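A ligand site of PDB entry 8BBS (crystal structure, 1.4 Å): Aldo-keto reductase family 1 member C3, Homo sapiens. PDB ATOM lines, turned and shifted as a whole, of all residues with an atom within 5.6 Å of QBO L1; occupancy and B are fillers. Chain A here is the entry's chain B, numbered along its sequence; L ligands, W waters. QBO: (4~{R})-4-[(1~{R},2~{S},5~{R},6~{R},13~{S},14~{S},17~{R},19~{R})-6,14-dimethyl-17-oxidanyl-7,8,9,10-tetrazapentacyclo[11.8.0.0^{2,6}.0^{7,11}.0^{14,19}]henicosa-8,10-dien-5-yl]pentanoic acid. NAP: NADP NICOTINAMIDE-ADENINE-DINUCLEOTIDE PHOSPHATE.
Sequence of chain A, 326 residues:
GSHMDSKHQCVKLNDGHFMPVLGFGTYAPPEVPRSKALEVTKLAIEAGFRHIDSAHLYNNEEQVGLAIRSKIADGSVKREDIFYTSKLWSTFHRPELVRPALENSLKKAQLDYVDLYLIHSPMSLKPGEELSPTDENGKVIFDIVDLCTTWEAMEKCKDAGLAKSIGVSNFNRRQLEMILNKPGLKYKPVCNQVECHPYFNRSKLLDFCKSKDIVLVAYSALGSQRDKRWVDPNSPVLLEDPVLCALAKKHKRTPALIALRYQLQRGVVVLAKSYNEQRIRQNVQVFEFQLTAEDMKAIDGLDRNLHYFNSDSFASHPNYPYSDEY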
ATOM      1  N   TYR A  27      19.881 -14.598   1.045  1.00  0.00           N
ATOM      2  CA  TYR A  27      19.051 -15.736   1.518  1.00  0.00           C
ATOM      3  C   TYR A  27      17.603 -15.290   1.596  1.00  0.00           C
ATOM      4  O   TYR A  27      17.282 -14.246   2.205  1.00  0.00           O
ATOM      5  CB  TYR A  27      19.482 -16.254   2.891  1.00  0.00           C
ATOM      6  CG  TYR A  27      18.568 -17.363   3.321  1.00  0.00           C
ATOM      7  CD1 TYR A  27      18.700 -18.607   2.748  1.00  0.00           C
ATOM      8  CD2 TYR A  27      17.548 -17.161   4.220  1.00  0.00           C
ATOM      9  CE1 TYR A  27      17.839 -19.649   3.072  1.00  0.00           C
ATOM     10  CE2 TYR A  27      16.669 -18.167   4.557  1.00  0.00           C
ATOM     11  CZ  TYR A  27      16.861 -19.440   4.019  1.00  0.00           C
ATOM     12  OH  TYR A  27      15.991 -20.460   4.322  1.00  0.00           O
ATOM     13  N   LEU A  57      23.782 -23.643   0.117  1.00  0.00           N
ATOM     14  CA  LEU A  57      22.599 -23.918   0.971  1.00  0.00           C
ATOM     15  C   LEU A  57      21.391 -23.084   0.520  1.00  0.00           C
ATOM     16  O   LEU A  57      20.243 -23.489   0.777  1.00  0.00           O
ATOM     17  CB  LEU A  57      22.977 -23.556   2.393  1.00  0.00           C
ATOM     18  CG  LEU A  57      21.877 -23.766   3.421  1.00  0.00           C
ATOM     19  CD1 LEU A  57      21.628 -25.236   3.553  1.00  0.00           C
ATOM     20  CD2 LEU A  57      22.256 -23.093   4.743  1.00  0.00           C
ATOM     21  N   TYR A  58      21.626 -21.885   0.005  1.00  0.00           N
ATOM     22  CA  TYR A  58      20.518 -20.926  -0.223  1.00  0.00           C
ATOM     23  C   TYR A  58      19.630 -21.333  -1.383  1.00  0.00           C
ATOM     24  O   TYR A  58      18.569 -20.709  -1.566  1.00  0.00           O
ATOM     25  CB  TYR A  58      21.042 -19.504  -0.414  1.00  0.00           C
ATOM     26  CG  TYR A  58      21.840 -18.961   0.722  1.00  0.00           C
ATOM     27  CD1 TYR A  58      21.927 -19.613   1.963  1.00  0.00           C
ATOM     28  CD2 TYR A  58      22.511 -17.745   0.575  1.00  0.00           C
ATOM     29  CE1 TYR A  58      22.673 -19.087   2.988  1.00  0.00           C
ATOM     30  CE2 TYR A  58      23.240 -17.205   1.622  1.00  0.00           C
ATOM     31  CZ  TYR A  58      23.368 -17.908   2.815  1.00  0.00           C
ATOM     32  OH  TYR A  58      24.135 -17.372   3.832  1.00  0.00           O
ATOM     33  N   LYS A  87      29.607 -20.305  -0.445  1.00  0.00           N
ATOM     34  CA  LYS A  87      30.025 -21.016   0.783  1.00  0.00           C
ATOM     35  C   LYS A  87      29.882 -22.510   0.592  1.00  0.00           C
ATOM     36  O   LYS A  87      28.895 -22.966  -0.007  1.00  0.00           O
ATOM     37  CB  LYS A  87      29.193 -20.571   1.995  1.00  0.00           C
ATOM     38  CG  LYS A  87      28.967 -19.074   2.095  1.00  0.00           C
ATOM     39  CD  LYS A  87      28.310 -18.665   3.396  1.00  0.00           C
ATOM     40  CE  LYS A  87      28.007 -17.185   3.459  1.00  0.00           C
ATOM     41  NZ  LYS A  87      26.782 -16.820   2.715  1.00  0.00           N
ATOM     42  N   TRP A  89      29.030 -25.961   1.960  1.00  0.00           N
ATOM     43  CA  TRP A  89      28.076 -26.479   2.956  1.00  0.00           C
ATOM     44  C   TRP A  89      28.758 -27.583   3.779  1.00  0.00           C
ATOM     45  O   TRP A  89      29.715 -28.172   3.342  1.00  0.00           O
ATOM     46  CB  TRP A  89      26.736 -26.890   2.316  1.00  0.00           C
ATOM     47  CG  TRP A  89      25.744 -27.311   3.366  1.00  0.00           C
ATOM     48  CD1 TRP A  89      25.158 -28.536   3.510  1.00  0.00           C
ATOM     49  CD2 TRP A  89      25.378 -26.549   4.537  1.00  0.00           C
ATOM     50  NE1 TRP A  89      24.423 -28.579   4.652  1.00  0.00           N
ATOM     51  CE2 TRP A  89      24.562 -27.391   5.339  1.00  0.00           C
ATOM     52  CE3 TRP A  89      25.684 -25.271   5.003  1.00  0.00           C
ATOM     53  CZ2 TRP A  89      24.027 -26.975   6.536  1.00  0.00           C
ATOM     54  CZ3 TRP A  89      25.159 -24.859   6.219  1.00  0.00           C
ATOM     55  CH2 TRP A  89      24.366 -25.716   6.986  1.00  0.00           C
ATOM     56  N   HIS A 120      31.138 -22.482   5.380  1.00  0.00           N
ATOM     57  CA  HIS A 120      29.869 -21.911   5.897  1.00  0.00           C
ATOM     58  C   HIS A 120      29.784 -22.007   7.424  1.00  0.00           C
ATOM     59  O   HIS A 120      29.287 -21.077   8.039  1.00  0.00           O
ATOM     60  CB  HIS A 120      28.672 -22.618   5.245  1.00  0.00           C
ATOM     61  CG  HIS A 120      27.411 -21.826   5.212  1.00  0.00           C
ATOM     62  ND1 HIS A 120      26.544 -21.887   4.150  1.00  0.00           N
ATOM     63  CD2 HIS A 120      26.854 -20.982   6.100  1.00  0.00           C
ATOM     64  CE1 HIS A 120      25.511 -21.117   4.388  1.00  0.00           C
ATOM     65  NE2 HIS A 120      25.682 -20.553   5.580  1.00  0.00           N
ATOM     66  N   LEU A 125      28.811 -32.032   8.932  1.00  0.00           N
ATOM     67  CA  LEU A 125      27.608 -32.904   8.888  1.00  0.00           C
ATOM     68  C   LEU A 125      27.926 -34.113   8.045  1.00  0.00           C
ATOM     69  O   LEU A 125      28.828 -34.088   7.195  1.00  0.00           O
ATOM     70  CB  LEU A 125      26.409 -32.148   8.317  1.00  0.00           C
ATOM     71  CG  LEU A 125      25.954 -30.932   9.096  1.00  0.00           C
ATOM     72  CD1 LEU A 125      24.776 -30.259   8.386  1.00  0.00           C
ATOM     73  CD2 LEU A 125      25.578 -31.301  10.517  1.00  0.00           C
ATOM     74  N   LEU A 131      21.664 -32.116   1.989  1.00  0.00           N
ATOM     75  CA  LEU A 131      22.198 -30.983   2.765  1.00  0.00           C
ATOM     76  C   LEU A 131      21.702 -31.034   4.198  1.00  0.00           C
ATOM     77  O   LEU A 131      22.356 -30.475   5.051  1.00  0.00           O
ATOM     78  CB  LEU A 131      21.788 -29.666   2.084  1.00  0.00           C
ATOM     79  CG  LEU A 131      22.298 -29.499   0.664  1.00  0.00           C
ATOM     80  CD1 LEU A 131      21.987 -28.105   0.163  1.00  0.00           C
ATOM     81  CD2 LEU A 131      23.779 -29.783   0.519  1.00  0.00           C
ATOM     82  N   SER A 132      20.627 -31.799   4.481  1.00  0.00           N
ATOM     83  CA  SER A 132      20.022 -31.922   5.821  1.00  0.00           C
ATOM     84  C   SER A 132      19.976 -33.397   6.189  1.00  0.00           C
ATOM     85  O   SER A 132      18.885 -33.973   6.238  1.00  0.00           O
ATOM     86  CB  SER A 132      18.642 -31.306   5.868  1.00  0.00           C
ATOM     87  OG  SER A 132      18.133 -31.318   7.184  1.00  0.00           O
ATOM     88  N   THR A 134      19.524 -36.580   8.313  1.00  0.00           N
ATOM     89  CA  THR A 134      18.819 -36.858   9.600  1.00  0.00           C
ATOM     90  C   THR A 134      18.702 -38.366   9.766  1.00  0.00           C
ATOM     91  O   THR A 134      18.665 -39.107   8.780  1.00  0.00           O
ATOM     92  CB  THR A 134      17.457 -36.148   9.693  1.00  0.00           C
ATOM     93  OG1 THR A 134      16.673 -36.551   8.560  1.00  0.00           O
ATOM     94  CG2 THR A 134      17.609 -34.646   9.734  1.00  0.00           C
ATOM     95  N   VAL A 140      19.736 -34.492  13.405  1.00  0.00           N
ATOM     96  CA  VAL A 140      20.795 -34.115  12.439  1.00  0.00           C
ATOM     97  C   VAL A 140      22.026 -34.973  12.694  1.00  0.00           C
ATOM     98  O   VAL A 140      22.406 -35.136  13.881  1.00  0.00           O
ATOM     99  CB  VAL A 140      21.149 -32.628  12.556  1.00  0.00           C
ATOM    100  CG1 VAL A 140      22.377 -32.271  11.738  1.00  0.00           C
ATOM    101  CG2 VAL A 140      19.962 -31.769  12.143  1.00  0.00           C
ATOM    102  N   TRP A 230      14.124 -20.894  13.134  1.00  0.00           N
ATOM    103  CA  TRP A 230      15.579 -20.722  13.434  1.00  0.00           C
ATOM    104  C   TRP A 230      15.793 -19.669  14.514  1.00  0.00           C
ATOM    105  O   TRP A 230      16.874 -19.676  15.073  1.00  0.00           O
ATOM    106  CB  TRP A 230      16.374 -20.365  12.163  1.00  0.00           C
ATOM    107  CG  TRP A 230      16.034 -21.189  10.967  1.00  0.00           C
ATOM    108  CD1 TRP A 230      15.587 -20.735   9.769  1.00  0.00           C
ATOM    109  CD2 TRP A 230      16.064 -22.631  10.874  1.00  0.00           C
ATOM    110  NE1 TRP A 230      15.313 -21.789   8.932  1.00  0.00           N
ATOM    111  CE2 TRP A 230      15.618 -22.959   9.574  1.00  0.00           C
ATOM    112  CE3 TRP A 230      16.448 -23.652  11.744  1.00  0.00           C
ATOM    113  CZ2 TRP A 230      15.474 -24.275   9.163  1.00  0.00           C
ATOM    114  CZ3 TRP A 230      16.298 -24.956  11.329  1.00  0.00           C
ATOM    115  CH2 TRP A 230      15.849 -25.254  10.049  1.00  0.00           C
ATOM    116  N   PHE A 309      20.401 -16.551  16.090  1.00  0.00           N
ATOM    117  CA  PHE A 309      20.586 -17.989  15.769  1.00  0.00           C
ATOM    118  C   PHE A 309      21.076 -18.737  17.014  1.00  0.00           C
ATOM    119  O   PHE A 309      22.182 -18.442  17.499  1.00  0.00           O
ATOM    120  CB  PHE A 309      21.496 -18.119  14.558  1.00  0.00           C
ATOM    121  CG  PHE A 309      20.858 -17.604  13.300  1.00  0.00           C
ATOM    122  CD1 PHE A 309      20.080 -18.433  12.516  1.00  0.00           C
ATOM    123  CD2 PHE A 309      21.053 -16.306  12.876  1.00  0.00           C
ATOM    124  CE1 PHE A 309      19.519 -17.986  11.325  1.00  0.00           C
ATOM    125  CE2 PHE A 309      20.421 -15.836  11.731  1.00  0.00           C
ATOM    126  CZ  PHE A 309      19.672 -16.672  10.951  1.00  0.00           C
ATOM    127  N   SER A 311      20.933 -22.247  16.976  1.00  0.00           N
ATOM    128  CA  SER A 311      21.451 -23.538  16.428  1.00  0.00           C
ATOM    129  C   SER A 311      21.012 -24.732  17.288  1.00  0.00           C
ATOM    130  O   SER A 311      21.889 -25.547  17.655  1.00  0.00           O
ATOM    131  CB  SER A 311      22.974 -23.531  16.331  1.00  0.00           C
ATOM    132  OG  SER A 311      23.465 -22.334  15.752  1.00  0.00           O
ATOM    133  N   SER A 313      19.306 -27.454  16.772  1.00  0.00           N
ATOM    134  CA  SER A 313      19.461 -28.781  16.086  1.00  0.00           C
ATOM    135  C   SER A 313      20.935 -29.226  16.041  1.00  0.00           C
ATOM    136  O   SER A 313      21.152 -30.419  15.776  1.00  0.00           O
ATOM    137  CB  SER A 313      18.826 -28.771  14.699  1.00  0.00           C
ATOM    138  OG  SER A 313      19.630 -28.089  13.751  1.00  0.00           O
ATOM    139  N   PHE A 314      21.897 -28.331  16.314  1.00  0.00           N
ATOM    140  CA  PHE A 314      23.344 -28.671  16.458  1.00  0.00           C
ATOM    141  C   PHE A 314      23.714 -28.821  17.938  1.00  0.00           C
ATOM    142  O   PHE A 314      24.918 -28.671  18.298  1.00  0.00           O
ATOM    143  CB  PHE A 314      24.263 -27.627  15.821  1.00  0.00           C
ATOM    144  CG  PHE A 314      24.052 -27.413  14.340  1.00  0.00           C
ATOM    145  CD1 PHE A 314      24.721 -28.195  13.408  1.00  0.00           C
ATOM    146  CD2 PHE A 314      23.214 -26.409  13.874  1.00  0.00           C
ATOM    147  CE1 PHE A 314      24.547 -27.981  12.042  1.00  0.00           C
ATOM    148  CE2 PHE A 314      23.042 -26.201  12.516  1.00  0.00           C
ATOM    149  CZ  PHE A 314      23.704 -26.998  11.599  1.00  0.00           C
HETATM  150  OBB QBO L   1      23.428 -18.573   5.939  1.00  0.00           O
HETATM  151  CBE QBO L   1      22.269 -18.160   6.214  1.00  0.00           C
HETATM  152  OBD QBO L   1      21.626 -17.176   5.716  1.00  0.00           O
HETATM  153  CAY QBO L   1      21.573 -18.850   7.383  1.00  0.00           C
HETATM  154  CAL QBO L   1      20.479 -19.794   6.892  1.00  0.00           C
HETATM  155  CAH QBO L   1      19.601 -20.144   8.128  1.00  0.00           C
HETATM  156  CAI QBO L   1      18.461 -19.160   8.192  1.00  0.00           C
HETATM  157  CAM QBO L   1      18.908 -21.560   8.128  1.00  0.00           C
HETATM  158  CAE QBO L   1      18.393 -21.928   6.704  1.00  0.00           C
HETATM  159  CAF QBO L   1      18.652 -23.435   6.533  1.00  0.00           C
HETATM  160  CAN QBO L   1      18.939 -23.960   7.893  1.00  0.00           C
HETATM  161  CAU QBO L   1      19.768 -22.792   8.566  1.00  0.00           C
HETATM  162  CAS QBO L   1      21.250 -22.703   8.086  1.00  0.00           C
HETATM  163  NBC QBO L   1      19.740 -22.870  10.039  1.00  0.00           N
HETATM  164  NAT QBO L   1      19.468 -21.816  10.851  1.00  0.00           N
HETATM  165  NAO QBO L   1      19.579 -22.223  12.137  1.00  0.00           N
HETATM  166  NAW QBO L   1      19.947 -23.557  12.029  1.00  0.00           N
HETATM  167  CAZ QBO L   1      20.008 -23.937  10.750  1.00  0.00           C
HETATM  168  CAV QBO L   1      20.403 -25.255  10.352  1.00  0.00           C
HETATM  169  CAG QBO L   1      19.501 -26.016   9.267  1.00  0.00           C
HETATM  170  CAA QBO L   1      19.511 -25.373   7.844  1.00  0.00           C
HETATM  171  CAC QBO L   1      18.618 -26.182   6.834  1.00  0.00           C
HETATM  172  CAD QBO L   1      18.982 -27.629   6.679  1.00  0.00           C
HETATM  173  CAB QBO L   1      18.949 -28.272   8.093  1.00  0.00           C
HETATM  174  CAR QBO L   1      17.492 -28.347   8.543  1.00  0.00           C
HETATM  175  CAX QBO L   1      17.505 -29.184   9.830  1.00  0.00           C
HETATM  176  OBA QBO L   1      16.132 -29.419  10.266  1.00  0.00           O
HETATM  177  CAQ QBO L   1      18.186 -28.457  10.881  1.00  0.00           C
HETATM  178  CAJ QBO L   1      19.638 -28.372  10.497  1.00  0.00           C
HETATM  179  CAP QBO L   1      19.838 -27.592   9.164  1.00  0.00           C
HETATM  180  CAK QBO L   1      21.300 -27.765   8.735  1.00  0.00           C
HETATM  181  PA  NAP L   2      19.345  -9.025   7.689  1.00  0.00           P
HETATM  182  O1A NAP L   2      20.347  -8.402   6.742  1.00  0.00           O
HETATM  183  O2A NAP L   2      19.557  -8.963   9.142  1.00  0.00           O
HETATM  184  O5B NAP L   2      17.948  -8.436   7.294  1.00  0.00           O
HETATM  185  C5B NAP L   2      16.806  -8.784   8.109  1.00  0.00           C
HETATM  186  C4B NAP L   2      15.552  -8.161   7.494  1.00  0.00           C
HETATM  187  O4B NAP L   2      15.724  -6.715   7.486  1.00  0.00           O
HETATM  188  C3B NAP L   2      15.314  -8.574   6.072  1.00  0.00           C
HETATM  189  O3B NAP L   2      14.464  -9.751   5.989  1.00  0.00           O
HETATM  190  C2B NAP L   2      14.665  -7.326   5.444  1.00  0.00           C
HETATM  191  O2B NAP L   2      13.295  -7.533   5.089  1.00  0.00           O
HETATM  192  C1B NAP L   2      14.795  -6.246   6.526  1.00  0.00           C
HETATM  193  N9A NAP L   2      15.326  -5.026   5.969  1.00  0.00           N
HETATM  194  C8A NAP L   2      16.352  -4.854   5.044  1.00  0.00           C
HETATM  195  N7A NAP L   2      16.556  -3.554   4.845  1.00  0.00           N
HETATM  196  C5A NAP L   2      15.689  -2.870   5.664  1.00  0.00           C
HETATM  197  C6A NAP L   2      15.409  -1.445   5.810  1.00  0.00           C
HETATM  198  N6A NAP L   2      16.135  -0.556   5.166  1.00  0.00           N
HETATM  199  N1A NAP L   2      14.479  -1.153   6.709  1.00  0.00           N
HETATM  200  C2A NAP L   2      13.753  -2.060   7.353  1.00  0.00           C
HETATM  201  N3A NAP L   2      13.947  -3.394   7.227  1.00  0.00           N
HETATM  202  C4A NAP L   2      14.897  -3.795   6.352  1.00  0.00           C
HETATM  203  O3  NAP L   2      19.086 -10.580   7.187  1.00  0.00           O
HETATM  204  PN  NAP L   2      19.898 -11.945   7.309  1.00  0.00           P
HETATM  205  O1N NAP L   2      19.383 -12.786   6.204  1.00  0.00           O
HETATM  206  O2N NAP L   2      19.822 -12.473   8.681  1.00  0.00           O
HETATM  207  O5D NAP L   2      21.416 -11.540   7.096  1.00  0.00           O
HETATM  208  C5D NAP L   2      21.841 -11.013   5.828  1.00  0.00           C
HETATM  209  C4D NAP L   2      22.587 -12.042   4.970  1.00  0.00           C
HETATM  210  O4D NAP L   2      23.718 -12.587   5.659  1.00  0.00           O
HETATM  211  C3D NAP L   2      21.792 -13.309   4.480  1.00  0.00           C
HETATM  212  O3D NAP L   2      20.832 -13.069   3.463  1.00  0.00           O
HETATM  213  C2D NAP L   2      22.930 -14.177   4.039  1.00  0.00           C
HETATM  214  O2D NAP L   2      23.454 -13.722   2.787  1.00  0.00           O
HETATM  215  C1D NAP L   2      23.962 -13.928   5.155  1.00  0.00           C
HETATM  216  N1N NAP L   2      23.853 -14.833   6.305  1.00  0.00           N
HETATM  217  C2N NAP L   2      24.820 -15.713   6.515  1.00  0.00           C
HETATM  218  C3N NAP L   2      24.832 -16.623   7.554  1.00  0.00           C
HETATM  219  C7N NAP L   2      25.979 -17.554   7.796  1.00  0.00           C
HETATM  220  O7N NAP L   2      25.793 -18.509   8.542  1.00  0.00           O
HETATM  221  N7N NAP L   2      27.160 -17.239   7.229  1.00  0.00           N
HETATM  222  C4N NAP L   2      23.789 -16.568   8.494  1.00  0.00           C
HETATM  223  C5N NAP L   2      22.753 -15.622   8.274  1.00  0.00           C
HETATM  224  C6N NAP L   2      22.855 -14.765   7.201  1.00  0.00           C
HETATM  225  P2B NAP L   2      12.824  -7.255   3.558  1.00  0.00           P
HETATM  226  O1X NAP L   2      13.406  -8.331   2.675  1.00  0.00           O
HETATM  227  O2X NAP L   2      11.288  -7.406   3.660  1.00  0.00           O
HETATM  228  O3X NAP L   2      13.323  -5.877   3.199  1.00  0.00           O
HETATM  229  O   HOH W   1      16.636 -16.323   7.575  1.00  0.00           O
HETATM  230  O   HOH W   2      19.263 -24.949  14.428  1.00  0.00           O
HETATM  231  O   HOH W   3      19.347 -15.763   6.728  1.00  0.00           O
HETATM  232  O   HOH W   4      19.111 -21.168  14.846  1.00  0.00           O
HETATM  233  O   HOH W   5      14.946 -32.119   9.685  1.00  0.00           O
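The backbone NH (N) of Tyr 27 lies within hydrogen-bond range of an oxygen (O3D) of NAP L2 (3.0 Å). An oxygen (OBB) of QBO L1 is in hydrogen-bond range of a ring nitrogen (NE2) of His 120. The side-chain hydroxyl (OH) of Tyr 58 sits at hydrogen-bond distance from an oxygen (OBB) of QBO L1 (2.5 Å).
OH of Tyr 58 lies within hydrogen-bond range of NZ of Lys 87 (2.9 Å). The indole nitrogen (NE1) of Trp 89 sits at hydrogen-bond distance from the backbone carbonyl oxygen (O) of Leu 131, at 2.8 Å.
CB of Tyr 27 touches OBD of QBO L1 (3.7 Å). Leu 57 touches QBO L1. CZ2 of Trp 89 touches CAK of QBO L1, 3.6 Å away. Ser 132 touches QBO L1. CG2 of Val 140 touches CAJ of QBO L1, at 3.8 Å. Trp 230 touches QBO L1. CE1 of Phe 309 touches CAI of QBO L1 (3.5 Å). Ser 313 touches QBO L1 (OG to CAQ, 3.2 Å). Phe 314 touches QBO L1 (CE2 to CAV, 3.5 Å). 11 residues have an atom within 4 Å of QBO L1: Tyr 27, Leu 57, Tyr 58, Trp 89, His 120, Ser 132, Val 140, Trp 230, Phe 309, Ser 313 and Phe 314.
Water W2 bridges NAW of QBO L1 (2.9 Å) and OG of Ser 313 (3.2 Å). Water W3 lies within hydrogen-bond range of OBD of QBO L1 and O1N of NAP L2. Water W4 lies within hydrogen-bond range of the backbone carbonyl oxygen (O) of Trp 230 (2.7 Å), a nitrogen (NAO) of QBO L1 (2.9 Å) and the backbone NH (N) of Ser 311 (3.0 Å).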
